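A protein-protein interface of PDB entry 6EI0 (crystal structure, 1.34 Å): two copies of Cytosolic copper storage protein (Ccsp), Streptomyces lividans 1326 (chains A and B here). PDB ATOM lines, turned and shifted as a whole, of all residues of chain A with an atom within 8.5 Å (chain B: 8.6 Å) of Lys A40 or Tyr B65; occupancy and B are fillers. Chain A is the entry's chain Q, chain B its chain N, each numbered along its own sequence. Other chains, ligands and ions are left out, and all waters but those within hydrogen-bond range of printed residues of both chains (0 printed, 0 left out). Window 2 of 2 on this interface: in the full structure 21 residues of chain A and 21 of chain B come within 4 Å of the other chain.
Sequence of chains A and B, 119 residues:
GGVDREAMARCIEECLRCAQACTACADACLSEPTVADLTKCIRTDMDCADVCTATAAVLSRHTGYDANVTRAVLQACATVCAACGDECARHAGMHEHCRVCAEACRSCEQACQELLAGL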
ATOM      1  N   CYS A  29      -2.867  12.044  11.343  1.00  0.00           N
ATOM      2  CA  CYS A  29      -2.559  12.712  12.613  1.00  0.00           C
ATOM      3  C   CYS A  29      -1.753  13.981  12.419  1.00  0.00           C
ATOM      4  O   CYS A  29      -1.989  14.972  13.097  1.00  0.00           O
ATOM      5  CB  CYS A  29      -1.801  11.795  13.557  1.00  0.00           C
ATOM      6  SG  CYS A  29      -2.755  10.409  14.258  1.00  0.00           S
ATOM      7  N   VAL A  35      -2.730  17.870  16.418  1.00  0.00           N
ATOM      8  CA  VAL A  35      -1.468  17.130  16.186  1.00  0.00           C
ATOM      9  C   VAL A  35      -0.579  17.067  17.443  1.00  0.00           C
ATOM     10  O   VAL A  35       0.047  16.021  17.691  1.00  0.00           O
ATOM     11  CB  VAL A  35      -0.675  17.679  14.977  1.00  0.00           C
ATOM     12  CG1 VAL A  35      -0.349  19.159  15.106  1.00  0.00           C
ATOM     13  CG2 VAL A  35       0.588  16.847  14.733  1.00  0.00           C
ATOM     14  N   ALA A  36      -0.548  18.123  18.261  1.00  0.00           N
ATOM     15  CA  ALA A  36       0.332  18.086  19.450  1.00  0.00           C
ATOM     16  C   ALA A  36      -0.005  16.983  20.454  1.00  0.00           C
ATOM     17  O   ALA A  36       0.879  16.506  21.154  1.00  0.00           O
ATOM     18  CB  ALA A  36       0.351  19.440  20.155  1.00  0.00           C
ATOM     19  N   ASP A  37      -1.272  16.577  20.495  1.00  0.00           N
ATOM     20  CA  ASP A  37      -1.757  15.493  21.356  1.00  0.00           C
ATOM     21  C   ASP A  37      -1.655  14.099  20.732  1.00  0.00           C
ATOM     22  O   ASP A  37      -2.068  13.101  21.363  1.00  0.00           O
ATOM     23  CB  ASP A  37      -3.226  15.754  21.701  1.00  0.00           C
ATOM     24  CG  ASP A  37      -3.444  17.124  22.303  1.00  0.00           C
ATOM     25  OD1 ASP A  37      -2.612  17.548  23.142  1.00  0.00           O
ATOM     26  OD2 ASP A  37      -4.447  17.786  21.938  1.00  0.00           O
ATOM     27  N   LEU A  38      -1.105  14.041  19.506  1.00  0.00           N
ATOM     28  CA  LEU A  38      -1.023  12.817  18.725  1.00  0.00           C
ATOM     29  C   LEU A  38       0.400  12.426  18.369  1.00  0.00           C
ATOM     30  O   LEU A  38       0.579  11.539  17.508  1.00  0.00           O
ATOM     31  CB  LEU A  38      -1.846  12.974  17.446  1.00  0.00           C
ATOM     32  CG  LEU A  38      -3.338  13.209  17.680  1.00  0.00           C
ATOM     33  CD1 LEU A  38      -3.994  13.642  16.375  1.00  0.00           C
ATOM     34  CD2 LEU A  38      -4.032  11.977  18.217  1.00  0.00           C
ATOM     35  N   THR A  39       1.401  13.058  18.988  1.00  0.00           N
ATOM     36  CA  THR A  39       2.772  12.824  18.588  1.00  0.00           C
ATOM     37  C   THR A  39       3.243  11.396  18.908  1.00  0.00           C
ATOM     38  O   THR A  39       4.036  10.833  18.131  1.00  0.00           O
ATOM     39  CB  THR A  39       3.776  13.833  19.200  1.00  0.00           C
ATOM     40  OG1 THR A  39       3.634  13.835  20.616  1.00  0.00           O
ATOM     41  CG2 THR A  39       3.560  15.237  18.673  1.00  0.00           C
ATOM     42  N   LYS A  40       2.776  10.799  20.015  1.00  0.00           N
ATOM     43  CA  LYS A  40       3.116   9.399  20.329  1.00  0.00           C
ATOM     44  C   LYS A  40       2.503   8.460  19.294  1.00  0.00           C
ATOM     45  O   LYS A  40       3.126   7.478  18.873  1.00  0.00           O
ATOM     46  CB  LYS A  40       2.664   8.972  21.733  1.00  0.00           C
ATOM     47  CG  LYS A  40       3.420   9.659  22.826  1.00  0.00           C
ATOM     48  CD  LYS A  40       2.902   9.271  24.208  1.00  0.00           C
ATOM     49  CE  LYS A  40       3.726   9.912  25.309  1.00  0.00           C
ATOM     50  NZ  LYS A  40       3.396  11.360  25.404  1.00  0.00           N
ATOM     51  N   CYS A  41       1.266   8.747  18.897  1.00  0.00           N
ATOM     52  CA  CYS A  41       0.594   7.979  17.853  1.00  0.00           C
ATOM     53  C   CYS A  41       1.366   8.020  16.546  1.00  0.00           C
ATOM     54  O   CYS A  41       1.612   6.957  15.942  1.00  0.00           O
ATOM     55  CB  CYS A  41      -0.820   8.488  17.654  1.00  0.00           C
ATOM     56  SG  CYS A  41      -1.835   7.434  16.626  1.00  0.00           S
ATOM     57  N   ILE A  42       1.795   9.218  16.143  1.00  0.00           N
ATOM     58  CA  ILE A  42       2.546   9.414  14.899  1.00  0.00           C
ATOM     59  C   ILE A  42       3.859   8.637  14.985  1.00  0.00           C
ATOM     60  O   ILE A  42       4.196   7.907  14.056  1.00  0.00           O
ATOM     61  CB  ILE A  42       2.848  10.909  14.637  1.00  0.00           C
ATOM     62  CG1 ILE A  42       1.559  11.666  14.324  1.00  0.00           C
ATOM     63  CG2 ILE A  42       3.891  11.092  13.536  1.00  0.00           C
ATOM     64  CD1 ILE A  42       1.692  13.158  14.447  1.00  0.00           C
ATOM     65  N   ARG A  43       4.586   8.760  16.098  1.00  0.00           N
ATOM     66  CA  ARG A  43       5.843   8.038  16.284  1.00  0.00           C
ATOM     67  C   ARG A  43       5.668   6.517  16.192  1.00  0.00           C
ATOM     68  O   ARG A  43       6.418   5.824  15.477  1.00  0.00           O
ATOM     69  CB  ARG A  43       6.468   8.403  17.616  1.00  0.00           C
ATOM     70  CG  ARG A  43       7.067   9.795  17.713  1.00  0.00           C
ATOM     71  CD  ARG A  43       7.482  10.075  19.145  1.00  0.00           C
ATOM     72  NE  ARG A  43       7.928  11.431  19.371  1.00  0.00           N
ATOM     73  CZ  ARG A  43       9.129  11.920  19.093  1.00  0.00           C
ATOM     74  NH1 ARG A  43      10.097  11.156  18.558  1.00  0.00           N
ATOM     75  NH2 ARG A  43       9.350  13.215  19.337  1.00  0.00           N
ATOM     76  N   THR A  44       4.675   5.995  16.896  1.00  0.00           N
ATOM     77  CA  THR A  44       4.474   4.559  16.925  1.00  0.00           C
ATOM     78  C   THR A  44       3.903   4.016  15.593  1.00  0.00           C
ATOM     79  O   THR A  44       4.241   2.887  15.193  1.00  0.00           O
ATOM     80  CB  THR A  44       3.634   4.145  18.150  1.00  0.00           C
ATOM     81  OG1 THR A  44       4.138   4.806  19.319  1.00  0.00           O
ATOM     82  CG2 THR A  44       3.709   2.676  18.380  1.00  0.00           C
ATOM     83  N   ASP A  45       3.073   4.805  14.912  1.00  0.00           N
ATOM     84  CA  ASP A  45       2.612   4.472  13.562  1.00  0.00           C
ATOM     85  C   ASP A  45       3.839   4.260  12.664  1.00  0.00           C
ATOM     86  O   ASP A  45       3.875   3.297  11.886  1.00  0.00           O
ATOM     87  CB  ASP A  45       1.809   5.634  13.011  1.00  0.00           C
ATOM     88  CG  ASP A  45       0.421   5.767  13.605  1.00  0.00           C
ATOM     89  OD1 ASP A  45      -0.119   4.824  14.237  1.00  0.00           O
ATOM     90  OD2 ASP A  45      -0.157   6.868  13.407  1.00  0.00           O
ATOM     91  N   MET A  46       4.801   5.180  12.714  1.00  0.00           N
ATOM     92  CA  MET A  46       5.979   5.065  11.867  1.00  0.00           C
ATOM     93  C   MET A  46       6.872   3.906  12.237  1.00  0.00           C
ATOM     94  O   MET A  46       7.401   3.202  11.366  1.00  0.00           O
ATOM     95  CB  MET A  46       6.719   6.380  11.803  1.00  0.00           C
ATOM     96  CG  MET A  46       5.866   7.460  11.152  1.00  0.00           C
ATOM     97  SD  MET A  46       5.120   6.936   9.561  1.00  0.00           S
ATOM     98  CE  MET A  46       6.508   6.326   8.592  1.00  0.00           C
ATOM     99  N   ASP A  47       7.009   3.654  13.530  1.00  0.00           N
ATOM    100  CA  ASP A  47       7.780   2.499  13.974  1.00  0.00           C
ATOM    101  C   ASP A  47       7.165   1.196  13.480  1.00  0.00           C
ATOM    102  O   ASP A  47       7.856   0.300  12.990  1.00  0.00           O
ATOM    103  CB  ASP A  47       7.830   2.435  15.507  1.00  0.00           C
ATOM    104  CG  ASP A  47       8.623   3.573  16.159  1.00  0.00           C
ATOM    105  OD1 ASP A  47       9.440   4.255  15.480  1.00  0.00           O
ATOM    106  OD2 ASP A  47       8.428   3.751  17.390  1.00  0.00           O
ATOM    107  N   ALA A  83       1.958  -2.207  20.455  1.00  0.00           N
ATOM    108  CA  ALA A  83       2.130  -0.827  20.963  1.00  0.00           C
ATOM    109  C   ALA A  83       1.340   0.173  20.106  1.00  0.00           C
ATOM    110  O   ALA A  83       0.706   1.090  20.626  1.00  0.00           O
ATOM    111  CB  ALA A  83       3.582  -0.449  20.969  1.00  0.00           C
ATOM    112  N   CYS A  84       1.468   0.024  18.799  1.00  0.00           N
ATOM    113  CA  CYS A  84       0.777   0.899  17.865  1.00  0.00           C
ATOM    114  C   CYS A  84      -0.754   0.793  18.002  1.00  0.00           C
ATOM    115  O   CYS A  84      -1.458   1.817  18.046  1.00  0.00           O
ATOM    116  CB  CYS A  84       1.220   0.650  16.415  1.00  0.00           C
ATOM    117  SG  CYS A  84       0.681   1.925  15.281  1.00  0.00           S
ATOM    118  N   ASP A  86      -2.399  -0.176  20.668  1.00  0.00           N
ATOM    119  CA  ASP A  86      -2.775   0.420  21.928  1.00  0.00           C
ATOM    120  C   ASP A  86      -2.836   1.920  21.831  1.00  0.00           C
ATOM    121  O   ASP A  86      -3.786   2.502  22.347  1.00  0.00           O
ATOM    122  CB  ASP A  86      -1.816   0.000  23.042  1.00  0.00           C
ATOM    123  CG  ASP A  86      -2.003  -1.456  23.444  1.00  0.00           C
ATOM    124  OD1 ASP A  86      -2.962  -2.108  22.955  1.00  0.00           O
ATOM    125  OD2 ASP A  86      -1.198  -1.972  24.247  1.00  0.00           O
ATOM    126  N   GLU A  87      -1.833   2.550  21.214  1.00  0.00           N
ATOM    127  CA  GLU A  87      -1.792   4.017  21.142  1.00  0.00           C
ATOM    128  C   GLU A  87      -2.913   4.561  20.242  1.00  0.00           C
ATOM    129  O   GLU A  87      -3.593   5.503  20.635  1.00  0.00           O
ATOM    130  CB  GLU A  87      -0.434   4.554  20.702  1.00  0.00           C
ATOM    131  CG  GLU A  87      -0.321   6.068  20.639  1.00  0.00           C
ATOM    132  CD  GLU A  87      -0.411   6.726  22.013  1.00  0.00           C
ATOM    133  OE1 GLU A  87       0.045   6.076  22.991  1.00  0.00           O
ATOM    134  OE2 GLU A  87      -0.919   7.869  22.099  1.00  0.00           O
ATOM    135  N   CYS A  88      -3.115   3.944  19.074  1.00  0.00           N
ATOM    136  CA  CYS A  88      -4.241   4.278  18.197  1.00  0.00           C
ATOM    137  C   CYS A  88      -5.593   4.093  18.883  1.00  0.00           C
ATOM    138  O   CYS A  88      -6.468   4.938  18.729  1.00  0.00           O
ATOM    139  CB  CYS A  88      -4.225   3.480  16.884  1.00  0.00           C
ATOM    140  SG  CYS A  88      -2.852   3.889  15.828  1.00  0.00           S
ATOM    141  N   ARG A  90      -6.385   4.482  21.940  1.00  0.00           N
ATOM    142  CA  ARG A  90      -6.604   5.657  22.829  1.00  0.00           C
ATOM    143  C   ARG A  90      -7.370   6.778  22.125  1.00  0.00           C
ATOM    144  O   ARG A  90      -8.027   7.589  22.805  1.00  0.00           O
ATOM    145  CB  ARG A  90      -5.294   6.312  23.301  1.00  0.00           C
ATOM    146  CG  ARG A  90      -4.392   5.556  24.255  1.00  0.00           C
ATOM    147  CD  ARG A  90      -3.219   6.458  24.688  1.00  0.00           C
ATOM    148  NE  ARG A  90      -3.512   7.420  25.788  1.00  0.00           N
ATOM    149  CZ  ARG A  90      -3.391   7.182  27.100  1.00  0.00           C
ATOM    150  NH1 ARG A  90      -3.029   5.996  27.514  1.00  0.00           N
ATOM    151  NH2 ARG A  90      -3.679   8.135  27.980  1.00  0.00           N
ATOM    152  N   HIS A  91      -7.196   6.874  20.794  1.00  0.00           N
ATOM    153  CA  HIS A  91      -7.721   7.984  20.002  1.00  0.00           C
ATOM    154  C   HIS A  91      -8.836   7.584  19.079  1.00  0.00           C
ATOM    155  O   HIS A  91      -9.339   8.428  18.356  1.00  0.00           O
ATOM    156  CB  HIS A  91      -6.597   8.651  19.211  1.00  0.00           C
ATOM    157  CG  HIS A  91      -5.429   9.033  20.059  1.00  0.00           C
ATOM    158  ND1 HIS A  91      -5.502   9.997  21.052  1.00  0.00           N
ATOM    159  CD2 HIS A  91      -4.182   8.517  20.131  1.00  0.00           C
ATOM    160  CE1 HIS A  91      -4.334  10.084  21.663  1.00  0.00           C
ATOM    161  NE2 HIS A  91      -3.516   9.195  21.129  1.00  0.00           N
ATOM    162  N   ARG B  61      13.203   7.942  16.873  1.00  0.00           N
ATOM    163  CA  ARG B  61      11.973   8.461  17.427  1.00  0.00           C
ATOM    164  C   ARG B  61      11.793   8.047  18.881  1.00  0.00           C
ATOM    165  O   ARG B  61      10.760   8.319  19.513  1.00  0.00           O
ATOM    166  CB  ARG B  61      10.801   7.971  16.587  1.00  0.00           C
ATOM    167  CG  ARG B  61      10.736   8.610  15.233  1.00  0.00           C
ATOM    168  CD  ARG B  61       9.528   8.104  14.471  1.00  0.00           C
ATOM    169  NE  ARG B  61       9.681   6.703  14.109  1.00  0.00           N
ATOM    170  CZ  ARG B  61      10.067   6.238  12.910  1.00  0.00           C
ATOM    171  NH1 ARG B  61      10.128   4.950  12.759  1.00  0.00           N
ATOM    172  NH2 ARG B  61      10.387   7.025  11.883  1.00  0.00           N
ATOM    173  N   HIS B  62      12.792   7.376  19.428  1.00  0.00           N
ATOM    174  CA  HIS B  62      12.738   6.986  20.816  1.00  0.00           C
ATOM    175  C   HIS B  62      12.734   8.245  21.725  1.00  0.00           C
ATOM    176  O   HIS B  62      13.503   9.202  21.553  1.00  0.00           O
ATOM    177  CB  HIS B  62      13.900   6.050  21.173  1.00  0.00           C
ATOM    178  CG  HIS B  62      14.035   5.768  22.642  1.00  0.00           C
ATOM    179  ND1 HIS B  62      13.441   4.678  23.259  1.00  0.00           N
ATOM    180  CD2 HIS B  62      14.704   6.433  23.625  1.00  0.00           C
ATOM    181  CE1 HIS B  62      13.702   4.713  24.550  1.00  0.00           C
ATOM    182  NE2 HIS B  62      14.485   5.752  24.801  1.00  0.00           N
ATOM    183  N   THR B  63      11.770   8.243  22.608  1.00  0.00           N
ATOM    184  CA  THR B  63      11.628   9.257  23.654  1.00  0.00           C
ATOM    185  C   THR B  63      11.806   8.728  25.053  1.00  0.00           C
ATOM    186  O   THR B  63      11.977   9.535  25.977  1.00  0.00           O
ATOM    187  CB  THR B  63      10.220   9.855  23.621  1.00  0.00           C
ATOM    188  OG1 THR B  63       9.277   8.833  23.994  1.00  0.00           O
ATOM    189  CG2 THR B  63       9.916  10.414  22.222  1.00  0.00           C
ATOM    190  N   GLY B  64      11.689   7.412  25.239  1.00  0.00           N
ATOM    191  CA  GLY B  64      11.671   6.815  26.581  1.00  0.00           C
ATOM    192  C   GLY B  64      10.301   6.274  26.955  1.00  0.00           C
ATOM    193  O   GLY B  64      10.182   5.425  27.836  1.00  0.00           O
ATOM    194  N   TYR B  65       9.261   6.773  26.291  1.00  0.00           N
ATOM    195  CA  TYR B  65       7.927   6.236  26.473  1.00  0.00           C
ATOM    196  C   TYR B  65       7.804   5.010  25.570  1.00  0.00           C
ATOM    197  O   TYR B  65       8.220   5.056  24.396  1.00  0.00           O
ATOM    198  CB  TYR B  65       6.855   7.273  26.127  1.00  0.00           C
ATOM    199  CG  TYR B  65       5.477   6.734  26.402  1.00  0.00           C
ATOM    200  CD1 TYR B  65       5.024   6.585  27.708  1.00  0.00           C
ATOM    201  CD2 TYR B  65       4.649   6.315  25.361  1.00  0.00           C
ATOM    202  CE1 TYR B  65       3.771   6.048  27.974  1.00  0.00           C
ATOM    203  CE2 TYR B  65       3.388   5.773  25.606  1.00  0.00           C
ATOM    204  CZ  TYR B  65       2.949   5.647  26.925  1.00  0.00           C
ATOM    205  OH  TYR B  65       1.698   5.128  27.206  1.00  0.00           O
ATOM    206  N   ASP B  66       7.204   3.942  26.105  1.00  0.00           N
ATOM    207  CA  ASP B  66       7.001   2.689  25.366  1.00  0.00           C
ATOM    208  C   ASP B  66       8.370   2.118  24.979  1.00  0.00           C
ATOM    209  O   ASP B  66       8.618   1.702  23.825  1.00  0.00           O
ATOM    210  N   ALA B  67       9.255   2.064  25.978  1.00  0.00           N
ATOM    211  CA  ALA B  67      10.599   1.540  25.756  1.00  0.00           C
ATOM    212  C   ALA B  67      10.626   0.043  25.362  1.00  0.00           C
ATOM    213  O   ALA B  67      11.655  -0.415  24.884  1.00  0.00           O
ATOM    214  CB  ALA B  67      11.511   1.823  26.944  1.00  0.00           C
ATOM    215  N   ASN B  68       9.515  -0.695  25.552  1.00  0.00           N
ATOM    216  CA  ASN B  68       9.461  -2.104  25.135  1.00  0.00           C
ATOM    217  C   ASN B  68       9.579  -2.239  23.619  1.00  0.00           C
ATOM    218  O   ASN B  68      10.149  -3.224  23.135  1.00  0.00           O
ATOM    219  CB  ASN B  68       8.239  -2.865  25.652  1.00  0.00           C
ATOM    220  CG  ASN B  68       6.925  -2.262  25.192  1.00  0.00           C
ATOM    221  OD1 ASN B  68       6.672  -1.075  25.407  1.00  0.00           O
ATOM    222  ND2 ASN B  68       6.063  -3.083  24.580  1.00  0.00           N
ATOM    223  N   VAL B  69       9.051  -1.263  22.873  1.00  0.00           N
ATOM    224  CA  VAL B  69       9.279  -1.230  21.424  1.00  0.00           C
ATOM    225  C   VAL B  69      10.780  -1.134  21.108  1.00  0.00           C
ATOM    226  O   VAL B  69      11.300  -1.870  20.269  1.00  0.00           O
ATOM    227  CB  VAL B  69       8.491  -0.058  20.772  1.00  0.00           C
ATOM    228  CG1 VAL B  69       8.959   0.224  19.333  1.00  0.00           C
ATOM    229  CG2 VAL B  69       6.994  -0.332  20.832  1.00  0.00           C
ATOM    230  N   THR B  70      11.452  -0.178  21.733  1.00  0.00           N
ATOM    231  CA  THR B  70      12.860   0.016  21.517  1.00  0.00           C
ATOM    232  C   THR B  70      13.652  -1.232  21.869  1.00  0.00           C
ATOM    233  O   THR B  70      14.505  -1.646  21.099  1.00  0.00           O
ATOM    234  CB  THR B  70      13.355   1.230  22.309  1.00  0.00           C
ATOM    235  OG1 THR B  70      12.563   2.374  21.915  1.00  0.00           O
ATOM    236  CG2 THR B  70      14.833   1.504  22.074  1.00  0.00           C
ATOM    237  N   LEU B 119      18.710   0.486  28.801  1.00  0.00           N
ATOM    238  CA  LEU B 119      17.261   0.473  28.948  1.00  0.00           C
ATOM    239  C   LEU B 119      16.928  -0.666  29.939  1.00  0.00           C
ATOM    240  O   LEU B 119      15.896  -0.665  30.564  1.00  0.00           O
ATOM    241  CB  LEU B 119      16.574   0.304  27.567  1.00  0.00           C
ATOM    242  CG  LEU B 119      16.910   1.355  26.496  1.00  0.00           C
ATOM    243  CD1 LEU B 119      16.457   0.870  25.124  1.00  0.00           C
ATOM    244  CD2 LEU B 119      16.315   2.735  26.759  1.00  0.00           C
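CD2 of Tyr B65 touches CD of Lys A40 (3.6 Å).
Arg A43 touches Thr B63.
Met A46 touches Arg B61.
Val B69 touches Ala A83.
No position is printed for both chains.
Of the 6 pairs that touch across the chains among the printed residues, none has its exchanged pair printed and touching as well.
NE of Arg B61 is in salt-bridge range of OD1 of Asp A47, at 2.8 Å.
The backbone carbonyl oxygen (O) of Arg B61 lies within hydrogen-bond range of the guanidinium group (NH1) of Arg A43.
Printed residues of chain B within 4 Å of Lys A40: Tyr B65 (3.6 Å).
Thr A44 touches none of the printed residues of chain B.
Of the printed residues of chain B, Met A46 touches Arg B61 (3.5 Å).
Of the printed residues of chain A, Arg B61 touches Arg A43 (3.1 Å), Met A46 (3.5 Å) and Asp A47 (2.8 Å).
No residue of chain A comes within 4 Å of Gly B64.
Of the printed residues of chain A, Val B69 touches Ala A83.
Thr B70 touches none of the printed residues of chain A.
The nearest printed residue of chain A that does not touch Tyr B65 is Glu A87 (4.3 Å).
The side-chain hydroxyl (OG1) of Thr B63 sits at hydrogen-bond distance from the backbone NH (N) of Tyr B65, 3.1 Å away.
O of Lys A40 lies within hydrogen-bond range of OG1 of Thr A44 (2.9 Å).
Printed residues of chain B that touch a printed residue of chain A: Arg B61, Thr B63, Tyr B65 and Val B69.
Among the printed residues, 6 pairs touch across the chains.
Among the printed residues, Asp or Glu carboxylates within 4 Å of a Lys or Arg side-chain nitrogen of the other chain: Asp A47 with Arg B61 (2.8 Å).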
